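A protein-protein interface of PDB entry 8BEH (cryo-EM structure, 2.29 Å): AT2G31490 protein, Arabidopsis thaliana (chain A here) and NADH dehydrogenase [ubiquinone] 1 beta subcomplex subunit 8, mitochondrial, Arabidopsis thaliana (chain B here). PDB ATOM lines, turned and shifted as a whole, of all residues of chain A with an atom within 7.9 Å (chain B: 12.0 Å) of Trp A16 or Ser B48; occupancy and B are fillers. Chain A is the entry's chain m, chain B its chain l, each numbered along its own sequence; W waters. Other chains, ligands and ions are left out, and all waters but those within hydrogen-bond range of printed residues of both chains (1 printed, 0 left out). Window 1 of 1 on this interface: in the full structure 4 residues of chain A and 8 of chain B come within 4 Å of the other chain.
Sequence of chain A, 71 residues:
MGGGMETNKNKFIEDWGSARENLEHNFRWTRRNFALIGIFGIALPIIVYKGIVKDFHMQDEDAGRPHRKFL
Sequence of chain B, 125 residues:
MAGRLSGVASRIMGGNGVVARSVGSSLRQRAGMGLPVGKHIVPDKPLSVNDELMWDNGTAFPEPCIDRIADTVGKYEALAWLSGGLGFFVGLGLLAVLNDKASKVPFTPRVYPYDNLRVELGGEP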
ATOM      1  N   ASN A  10      30.942  11.588  12.782  1.00  0.00           N
ATOM      2  CA  ASN A  10      29.761  10.747  12.908  1.00  0.00           C
ATOM      3  C   ASN A  10      28.689  11.299  11.979  1.00  0.00           C
ATOM      4  O   ASN A  10      28.388  12.495  12.018  1.00  0.00           O
ATOM      5  CB  ASN A  10      29.257  10.710  14.352  1.00  0.00           C
ATOM      6  CG  ASN A  10      27.918  10.013  14.488  1.00  0.00           C
ATOM      7  OD1 ASN A  10      26.867  10.628  14.338  1.00  0.00           O
ATOM      8  ND2 ASN A  10      27.953   8.724  14.790  1.00  0.00           N
ATOM      9  N   LYS A  11      28.114  10.425  11.152  1.00  0.00           N
ATOM     10  CA  LYS A  11      27.217  10.881  10.093  1.00  0.00           C
ATOM     11  C   LYS A  11      25.973  11.555  10.660  1.00  0.00           C
ATOM     12  O   LYS A  11      25.492  12.549  10.109  1.00  0.00           O
ATOM     13  CB  LYS A  11      26.844   9.708   9.185  1.00  0.00           C
ATOM     14  CG  LYS A  11      25.437   9.750   8.622  1.00  0.00           C
ATOM     15  CD  LYS A  11      25.275   8.755   7.477  1.00  0.00           C
ATOM     16  CE  LYS A  11      23.857   8.223   7.392  1.00  0.00           C
ATOM     17  NZ  LYS A  11      23.437   7.566   8.657  1.00  0.00           N
ATOM     18  N   PHE A  12      25.441  11.032  11.763  1.00  0.00           N
ATOM     19  CA  PHE A  12      24.236  11.612  12.348  1.00  0.00           C
ATOM     20  C   PHE A  12      24.515  12.969  12.985  1.00  0.00           C
ATOM     21  O   PHE A  12      23.686  13.879  12.900  1.00  0.00           O
ATOM     22  CB  PHE A  12      23.645  10.642  13.363  1.00  0.00           C
ATOM     23  CG  PHE A  12      23.355   9.289  12.792  1.00  0.00           C
ATOM     24  CD1 PHE A  12      22.150   9.039  12.162  1.00  0.00           C
ATOM     25  CD2 PHE A  12      24.297   8.274  12.860  1.00  0.00           C
ATOM     26  CE1 PHE A  12      21.877   7.797  11.633  1.00  0.00           C
ATOM     27  CE2 PHE A  12      24.028   7.030  12.327  1.00  0.00           C
ATOM     28  CZ  PHE A  12      22.818   6.795  11.710  1.00  0.00           C
ATOM     29  N   ILE A  13      25.680  13.124  13.618  1.00  0.00           N
ATOM     30  CA  ILE A  13      26.051  14.407  14.208  1.00  0.00           C
ATOM     31  C   ILE A  13      26.218  15.466  13.123  1.00  0.00           C
ATOM     32  O   ILE A  13      25.754  16.605  13.266  1.00  0.00           O
ATOM     33  CB  ILE A  13      27.326  14.243  15.056  1.00  0.00           C
ATOM     34  CG1 ILE A  13      27.031  13.382  16.283  1.00  0.00           C
ATOM     35  CG2 ILE A  13      27.872  15.588  15.482  1.00  0.00           C
ATOM     36  CD1 ILE A  13      28.267  12.976  17.043  1.00  0.00           C
ATOM     37  N   GLU A  14      26.863  15.104  12.015  1.00  0.00           N
ATOM     38  CA  GLU A  14      27.003  16.043  10.906  1.00  0.00           C
ATOM     39  C   GLU A  14      25.664  16.344  10.243  1.00  0.00           C
ATOM     40  O   GLU A  14      25.424  17.483   9.830  1.00  0.00           O
ATOM     41  CB  GLU A  14      28.014  15.513   9.894  1.00  0.00           C
ATOM     42  CG  GLU A  14      29.347  15.224  10.530  1.00  0.00           C
ATOM     43  CD  GLU A  14      30.157  16.490  10.733  1.00  0.00           C
ATOM     44  OE1 GLU A  14      31.054  16.493  11.597  1.00  0.00           O
ATOM     45  OE2 GLU A  14      29.894  17.487  10.031  1.00  0.00           O
ATOM     46  N   ASP A  15      24.782  15.347  10.132  1.00  0.00           N
ATOM     47  CA  ASP A  15      23.443  15.607   9.612  1.00  0.00           C
ATOM     48  C   ASP A  15      22.696  16.595  10.494  1.00  0.00           C
ATOM     49  O   ASP A  15      22.050  17.521   9.997  1.00  0.00           O
ATOM     50  CB  ASP A  15      22.654  14.302   9.497  1.00  0.00           C
ATOM     51  CG  ASP A  15      23.092  13.463   8.327  1.00  0.00           C
ATOM     52  OD1 ASP A  15      22.905  12.230   8.370  1.00  0.00           O
ATOM     53  OD2 ASP A  15      23.636  14.038   7.363  1.00  0.00           O
ATOM     54  N   TRP A  16      22.784  16.410  11.812  1.00  0.00           N
ATOM     55  CA  TRP A  16      22.174  17.328  12.767  1.00  0.00           C
ATOM     56  C   TRP A  16      22.724  18.743  12.604  1.00  0.00           C
ATOM     57  O   TRP A  16      21.961  19.718  12.529  1.00  0.00           O
ATOM     58  CB  TRP A  16      22.430  16.780  14.168  1.00  0.00           C
ATOM     59  CG  TRP A  16      21.903  17.540  15.330  1.00  0.00           C
ATOM     60  CD1 TRP A  16      20.603  17.820  15.614  1.00  0.00           C
ATOM     61  CD2 TRP A  16      22.677  18.090  16.394  1.00  0.00           C
ATOM     62  NE1 TRP A  16      20.518  18.516  16.793  1.00  0.00           N
ATOM     63  CE2 TRP A  16      21.781  18.696  17.291  1.00  0.00           C
ATOM     64  CE3 TRP A  16      24.047  18.132  16.673  1.00  0.00           C
ATOM     65  CZ2 TRP A  16      22.207  19.342  18.448  1.00  0.00           C
ATOM     66  CZ3 TRP A  16      24.468  18.769  17.820  1.00  0.00           C
ATOM     67  CH2 TRP A  16      23.551  19.364  18.694  1.00  0.00           C
ATOM     68  N   GLY A  17      24.049  18.869  12.503  1.00  0.00           N
ATOM     69  CA  GLY A  17      24.650  20.183  12.326  1.00  0.00           C
ATOM     70  C   GLY A  17      24.239  20.864  11.032  1.00  0.00           C
ATOM     71  O   GLY A  17      23.883  22.048  11.027  1.00  0.00           O
ATOM     72  N   SER A  18      24.270  20.126   9.919  1.00  0.00           N
ATOM     73  CA  SER A  18      23.897  20.713   8.636  1.00  0.00           C
ATOM     74  C   SER A  18      22.416  21.067   8.589  1.00  0.00           C
ATOM     75  O   SER A  18      22.043  22.070   7.975  1.00  0.00           O
ATOM     76  CB  SER A  18      24.262  19.771   7.488  1.00  0.00           C
ATOM     77  OG  SER A  18      23.889  18.436   7.766  1.00  0.00           O
ATOM     78  N   ALA A  19      21.561  20.269   9.233  1.00  0.00           N
ATOM     79  CA  ALA A  19      20.156  20.637   9.346  1.00  0.00           C
ATOM     80  C   ALA A  19      20.000  21.941  10.115  1.00  0.00           C
ATOM     81  O   ALA A  19      19.175  22.788   9.756  1.00  0.00           O
ATOM     82  CB  ALA A  19      19.367  19.519  10.023  1.00  0.00           C
ATOM     83  N   ARG A  20      20.833  22.127  11.143  1.00  0.00           N
ATOM     84  CA  ARG A  20      20.808  23.398  11.915  1.00  0.00           C
ATOM     85  C   ARG A  20      21.219  24.554  10.996  1.00  0.00           C
ATOM     86  O   ARG A  20      20.591  25.628  11.091  1.00  0.00           O
ATOM     87  CB  ARG A  20      21.734  23.298  13.132  1.00  0.00           C
ATOM     88  CG  ARG A  20      21.744  24.536  14.017  1.00  0.00           C
ATOM     89  CD  ARG A  20      20.368  24.912  14.536  1.00  0.00           C
ATOM     90  NE  ARG A  20      19.726  23.835  15.280  1.00  0.00           N
ATOM     91  CZ  ARG A  20      19.910  23.581  16.571  1.00  0.00           C
ATOM     92  NH1 ARG A  20      20.733  24.324  17.290  1.00  0.00           N
ATOM     93  NH2 ARG A  20      19.273  22.574  17.138  1.00  0.00           N
ATOM     94  N   GLU A  21      22.217  24.340  10.129  1.00  0.00           N
ATOM     95  CA  GLU A  21      22.703  25.429   9.283  1.00  0.00           C
ATOM     96  C   GLU A  21      21.752  25.807   8.149  1.00  0.00           C
ATOM     97  O   GLU A  21      21.964  26.845   7.518  1.00  0.00           O
ATOM     98  CB  GLU A  21      24.068  25.083   8.676  1.00  0.00           C
ATOM     99  CG  GLU A  21      25.137  24.728   9.676  1.00  0.00           C
ATOM    100  CD  GLU A  21      26.005  23.572   9.217  1.00  0.00           C
ATOM    101  OE1 GLU A  21      26.788  23.057  10.038  1.00  0.00           O
ATOM    102  OE2 GLU A  21      25.910  23.179   8.037  1.00  0.00           O
ATOM    103  N   ASN A  22      20.722  25.017   7.869  1.00  0.00           N
ATOM    104  CA  ASN A  22      19.873  25.242   6.706  1.00  0.00           C
ATOM    105  C   ASN A  22      18.401  25.340   7.089  1.00  0.00           C
ATOM    106  O   ASN A  22      17.518  24.884   6.364  1.00  0.00           O
ATOM    107  CB  ASN A  22      20.095  24.149   5.666  1.00  0.00           C
ATOM    108  CG  ASN A  22      21.531  24.085   5.201  1.00  0.00           C
ATOM    109  OD1 ASN A  22      22.194  23.059   5.325  1.00  0.00           O
ATOM    110  ND2 ASN A  22      22.025  25.193   4.674  1.00  0.00           N
ATOM    111  N   ILE B  41      28.312   6.706  24.326  1.00  0.00           N
ATOM    112  CA  ILE B  41      27.461   6.151  23.281  1.00  0.00           C
ATOM    113  C   ILE B  41      27.597   7.005  22.031  1.00  0.00           C
ATOM    114  O   ILE B  41      27.424   8.229  22.073  1.00  0.00           O
ATOM    115  CB  ILE B  41      26.001   6.075  23.751  1.00  0.00           C
ATOM    116  CG1 ILE B  41      25.936   5.606  25.206  1.00  0.00           C
ATOM    117  CG2 ILE B  41      25.210   5.138  22.854  1.00  0.00           C
ATOM    118  CD1 ILE B  41      24.800   6.213  25.990  1.00  0.00           C
ATOM    119  N   VAL B  42      27.931   6.364  20.918  1.00  0.00           N
ATOM    120  CA  VAL B  42      28.034   7.038  19.628  1.00  0.00           C
ATOM    121  C   VAL B  42      26.700   6.861  18.913  1.00  0.00           C
ATOM    122  O   VAL B  42      26.238   5.723  18.753  1.00  0.00           O
ATOM    123  CB  VAL B  42      29.208   6.491  18.804  1.00  0.00           C
ATOM    124  CG1 VAL B  42      29.048   6.858  17.350  1.00  0.00           C
ATOM    125  CG2 VAL B  42      30.516   7.009  19.351  1.00  0.00           C
ATOM    126  N   PRO B  43      26.049   7.941  18.487  1.00  0.00           N
ATOM    127  CA  PRO B  43      24.679   7.829  17.967  1.00  0.00           C
ATOM    128  C   PRO B  43      24.584   6.889  16.772  1.00  0.00           C
ATOM    129  O   PRO B  43      25.457   6.867  15.903  1.00  0.00           O
ATOM    130  CB  PRO B  43      24.334   9.268  17.574  1.00  0.00           C
ATOM    131  CG  PRO B  43      25.222  10.117  18.411  1.00  0.00           C
ATOM    132  CD  PRO B  43      26.490   9.342  18.604  1.00  0.00           C
ATOM    133  N   ASP B  44      23.505   6.107  16.742  1.00  0.00           N
ATOM    134  CA  ASP B  44      23.186   5.253  15.606  1.00  0.00           C
ATOM    135  C   ASP B  44      21.865   5.619  14.945  1.00  0.00           C
ATOM    136  O   ASP B  44      21.493   4.990  13.950  1.00  0.00           O
ATOM    137  CB  ASP B  44      23.153   3.781  16.030  1.00  0.00           C
ATOM    138  CG  ASP B  44      22.362   3.558  17.300  1.00  0.00           C
ATOM    139  OD1 ASP B  44      21.124   3.713  17.272  1.00  0.00           O
ATOM    140  OD2 ASP B  44      22.982   3.224  18.331  1.00  0.00           O
ATOM    141  N   LYS B  45      21.155   6.609  15.460  1.00  0.00           N
ATOM    142  CA  LYS B  45      19.896   7.100  14.925  1.00  0.00           C
ATOM    143  C   LYS B  45      20.012   8.599  14.715  1.00  0.00           C
ATOM    144  O   LYS B  45      20.847   9.255  15.345  1.00  0.00           O
ATOM    145  CB  LYS B  45      18.728   6.802  15.877  1.00  0.00           C
ATOM    146  CG  LYS B  45      18.534   5.337  16.210  1.00  0.00           C
ATOM    147  CD  LYS B  45      17.451   5.086  17.269  1.00  0.00           C
ATOM    148  CE  LYS B  45      17.346   6.151  18.374  1.00  0.00           C
ATOM    149  NZ  LYS B  45      18.634   6.736  18.857  1.00  0.00           N
ATOM    150  N   PRO B  46      19.209   9.171  13.820  1.00  0.00           N
ATOM    151  CA  PRO B  46      19.235  10.629  13.644  1.00  0.00           C
ATOM    152  C   PRO B  46      18.885  11.349  14.938  1.00  0.00           C
ATOM    153  O   PRO B  46      17.942  10.983  15.640  1.00  0.00           O
ATOM    154  CB  PRO B  46      18.190  10.873  12.552  1.00  0.00           C
ATOM    155  CG  PRO B  46      18.124   9.579  11.809  1.00  0.00           C
ATOM    156  CD  PRO B  46      18.342   8.512  12.829  1.00  0.00           C
ATOM    157  N   LEU B  47      19.671  12.371  15.254  1.00  0.00           N
ATOM    158  CA  LEU B  47      19.413  13.169  16.439  1.00  0.00           C
ATOM    159  C   LEU B  47      18.221  14.088  16.210  1.00  0.00           C
ATOM    160  O   LEU B  47      17.934  14.507  15.085  1.00  0.00           O
ATOM    161  CB  LEU B  47      20.644  13.989  16.810  1.00  0.00           C
ATOM    162  CG  LEU B  47      21.938  13.194  16.970  1.00  0.00           C
ATOM    163  CD1 LEU B  47      23.121  14.125  17.123  1.00  0.00           C
ATOM    164  CD2 LEU B  47      21.832  12.247  18.141  1.00  0.00           C
ATOM    165  N   SER B  48      17.514  14.388  17.295  1.00  0.00           N
ATOM    166  CA  SER B  48      16.411  15.330  17.241  1.00  0.00           C
ATOM    167  C   SER B  48      16.940  16.762  17.216  1.00  0.00           C
ATOM    168  O   SER B  48      18.131  17.018  17.411  1.00  0.00           O
ATOM    169  CB  SER B  48      15.472  15.131  18.427  1.00  0.00           C
ATOM    170  OG  SER B  48      16.192  14.815  19.605  1.00  0.00           O
ATOM    171  N   VAL B  49      16.029  17.704  16.973  1.00  0.00           N
ATOM    172  CA  VAL B  49      16.403  19.114  16.941  1.00  0.00           C
ATOM    173  C   VAL B  49      16.821  19.598  18.325  1.00  0.00           C
ATOM    174  O   VAL B  49      17.804  20.333  18.466  1.00  0.00           O
ATOM    175  CB  VAL B  49      15.253  19.959  16.363  1.00  0.00           C
ATOM    176  CG1 VAL B  49      15.074  19.652  14.885  1.00  0.00           C
ATOM    177  CG2 VAL B  49      13.961  19.691  17.109  1.00  0.00           C
ATOM    178  N   ASN B  50      16.084  19.211  19.361  1.00  0.00           N
ATOM    179  CA  ASN B  50      16.400  19.623  20.725  1.00  0.00           C
ATOM    180  C   ASN B  50      17.087  18.478  21.464  1.00  0.00           C
ATOM    181  O   ASN B  50      16.533  17.836  22.355  1.00  0.00           O
ATOM    182  CB  ASN B  50      15.139  20.091  21.442  1.00  0.00           C
ATOM    183  CG  ASN B  50      14.658  21.436  20.946  1.00  0.00           C
ATOM    184  OD1 ASN B  50      14.774  21.754  19.761  1.00  0.00           O
ATOM    185  ND2 ASN B  50      14.125  22.244  21.853  1.00  0.00           N
ATOM    186  N   ASP B  51      18.335  18.240  21.069  1.00  0.00           N
ATOM    187  CA  ASP B  51      19.163  17.203  21.664  1.00  0.00           C
ATOM    188  C   ASP B  51      20.332  17.773  22.451  1.00  0.00           C
ATOM    189  O   ASP B  51      20.947  17.044  23.234  1.00  0.00           O
ATOM    190  CB  ASP B  51      19.685  16.260  20.570  1.00  0.00           C
ATOM    191  CG  ASP B  51      20.247  14.972  21.126  1.00  0.00           C
ATOM    192  OD1 ASP B  51      19.902  14.607  22.271  1.00  0.00           O
ATOM    193  OD2 ASP B  51      21.037  14.320  20.413  1.00  0.00           O
ATOM    194  N   GLU B  52      20.642  19.058  22.269  1.00  0.00           N
ATOM    195  CA  GLU B  52      21.713  19.699  23.019  1.00  0.00           C
ATOM    196  C   GLU B  52      21.408  19.791  24.506  1.00  0.00           C
ATOM    197  O   GLU B  52      22.334  19.976  25.302  1.00  0.00           O
ATOM    198  CB  GLU B  52      21.960  21.102  22.476  1.00  0.00           C
ATOM    199  CG  GLU B  52      20.710  21.959  22.474  1.00  0.00           C
ATOM    200  CD  GLU B  52      20.204  22.242  21.086  1.00  0.00           C
ATOM    201  OE1 GLU B  52      19.807  21.281  20.392  1.00  0.00           O
ATOM    202  OE2 GLU B  52      20.192  23.424  20.693  1.00  0.00           O
ATOM    203  N   LEU B  53      20.137  19.681  24.896  1.00  0.00           N
ATOM    204  CA  LEU B  53      19.726  19.901  26.274  1.00  0.00           C
ATOM    205  C   LEU B  53      19.094  18.686  26.936  1.00  0.00           C
ATOM    206  O   LEU B  53      18.718  18.772  28.111  1.00  0.00           O
ATOM    207  CB  LEU B  53      18.750  21.087  26.355  1.00  0.00           C
ATOM    208  CG  LEU B  53      17.625  21.242  25.325  1.00  0.00           C
ATOM    209  CD1 LEU B  53      16.516  20.222  25.520  1.00  0.00           C
ATOM    210  CD2 LEU B  53      17.059  22.648  25.359  1.00  0.00           C
ATOM    211  N   MET B  54      18.959  17.568  26.235  1.00  0.00           N
ATOM    212  CA  MET B  54      18.285  16.403  26.800  1.00  0.00           C
ATOM    213  C   MET B  54      19.286  15.422  27.399  1.00  0.00           C
ATOM    214  O   MET B  54      19.094  14.928  28.510  1.00  0.00           O
ATOM    215  CB  MET B  54      17.434  15.707  25.737  1.00  0.00           C
ATOM    216  CG  MET B  54      15.937  15.950  25.881  1.00  0.00           C
ATOM    217  SD  MET B  54      15.315  15.557  27.526  1.00  0.00           S
ATOM    218  CE  MET B  54      14.954  13.811  27.345  1.00  0.00           C
HETATM  219  O   HOH W   1      21.107  13.319  12.865  1.00  0.00           O
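Hydrophobic or aromatic side chains of chain B within 4 Å of the printed part of chain A: Val B42 and Pro B46. Printed residues of chain A that touch a printed residue of chain B: Asn A10, Phe A12, Trp A16 and Arg A20. Hydrophobic or aromatic side chains of chain A within 4 Å of the printed part of chain B: Phe A12 and Trp A16. Among the printed residues, 11 pairs touch across the chains. Among the printed residues, Asp or Glu carboxylates within 4 Å of a Lys or Arg side-chain nitrogen of the other chain: Arg A20 with Glu B52 (3.5 Å).
O of Pro B43 sits at hydrogen-bond distance from ND2 of Asn A10 (3.3 Å). The backbone carbonyl oxygen (O) of Ser B48 is in hydrogen-bond range of the indole nitrogen (NE1) of Trp A16 (2.9 Å). The guanidinium group (NH2) of Arg A20 is in hydrogen-bond range of the backbone carbonyl oxygen (O) of Val B49, at 3.0 Å. NH2 of Arg A20 is in salt-bridge range of OE1 of Glu B52, at 3.5 Å.
The side-chain amide oxygen (OD1) of Asn A10 is in hydrogen-bond range of the backbone NH (N) of Phe A12. OD1 of Asn A10 sits at hydrogen-bond distance from N of Ile A13.
Among the printed residues, merely in contact across the chains: Phe A12 with Asp B44, Asn A10 with Val B42, Phe A12 with Lys B45, Phe A12 with Pro B46, Phe A12 with Pro B43, Trp A16 with Glu B52 and Trp A16 with Val B49.
Water W1 lies within hydrogen-bond range of O of Phe A12 (2.6 Å) and N of Leu B47 (2.9 Å).
Printed residues of chain B within 4 Å of Phe A12: Pro B43, Asp B44, Lys B45 and Pro B46. No residue of chain B comes within 4 Å of Asp A15. Of the printed residues of chain B, Trp A16 touches Ser B48, Val B49 and Glu B52. Gly A17 touches none of the printed residues of chain B. No residue of chain B comes within 4 Å of Ala A19. Glu A21 touches none of the printed residues of chain B. Of the printed residues of chain A, Pro B43 touches Asn A10 and Phe A12. Leu B47 touches none of the printed residues of chain A. Ser B48 touches just one residue of chain A: Trp A16 (2.9 Å).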
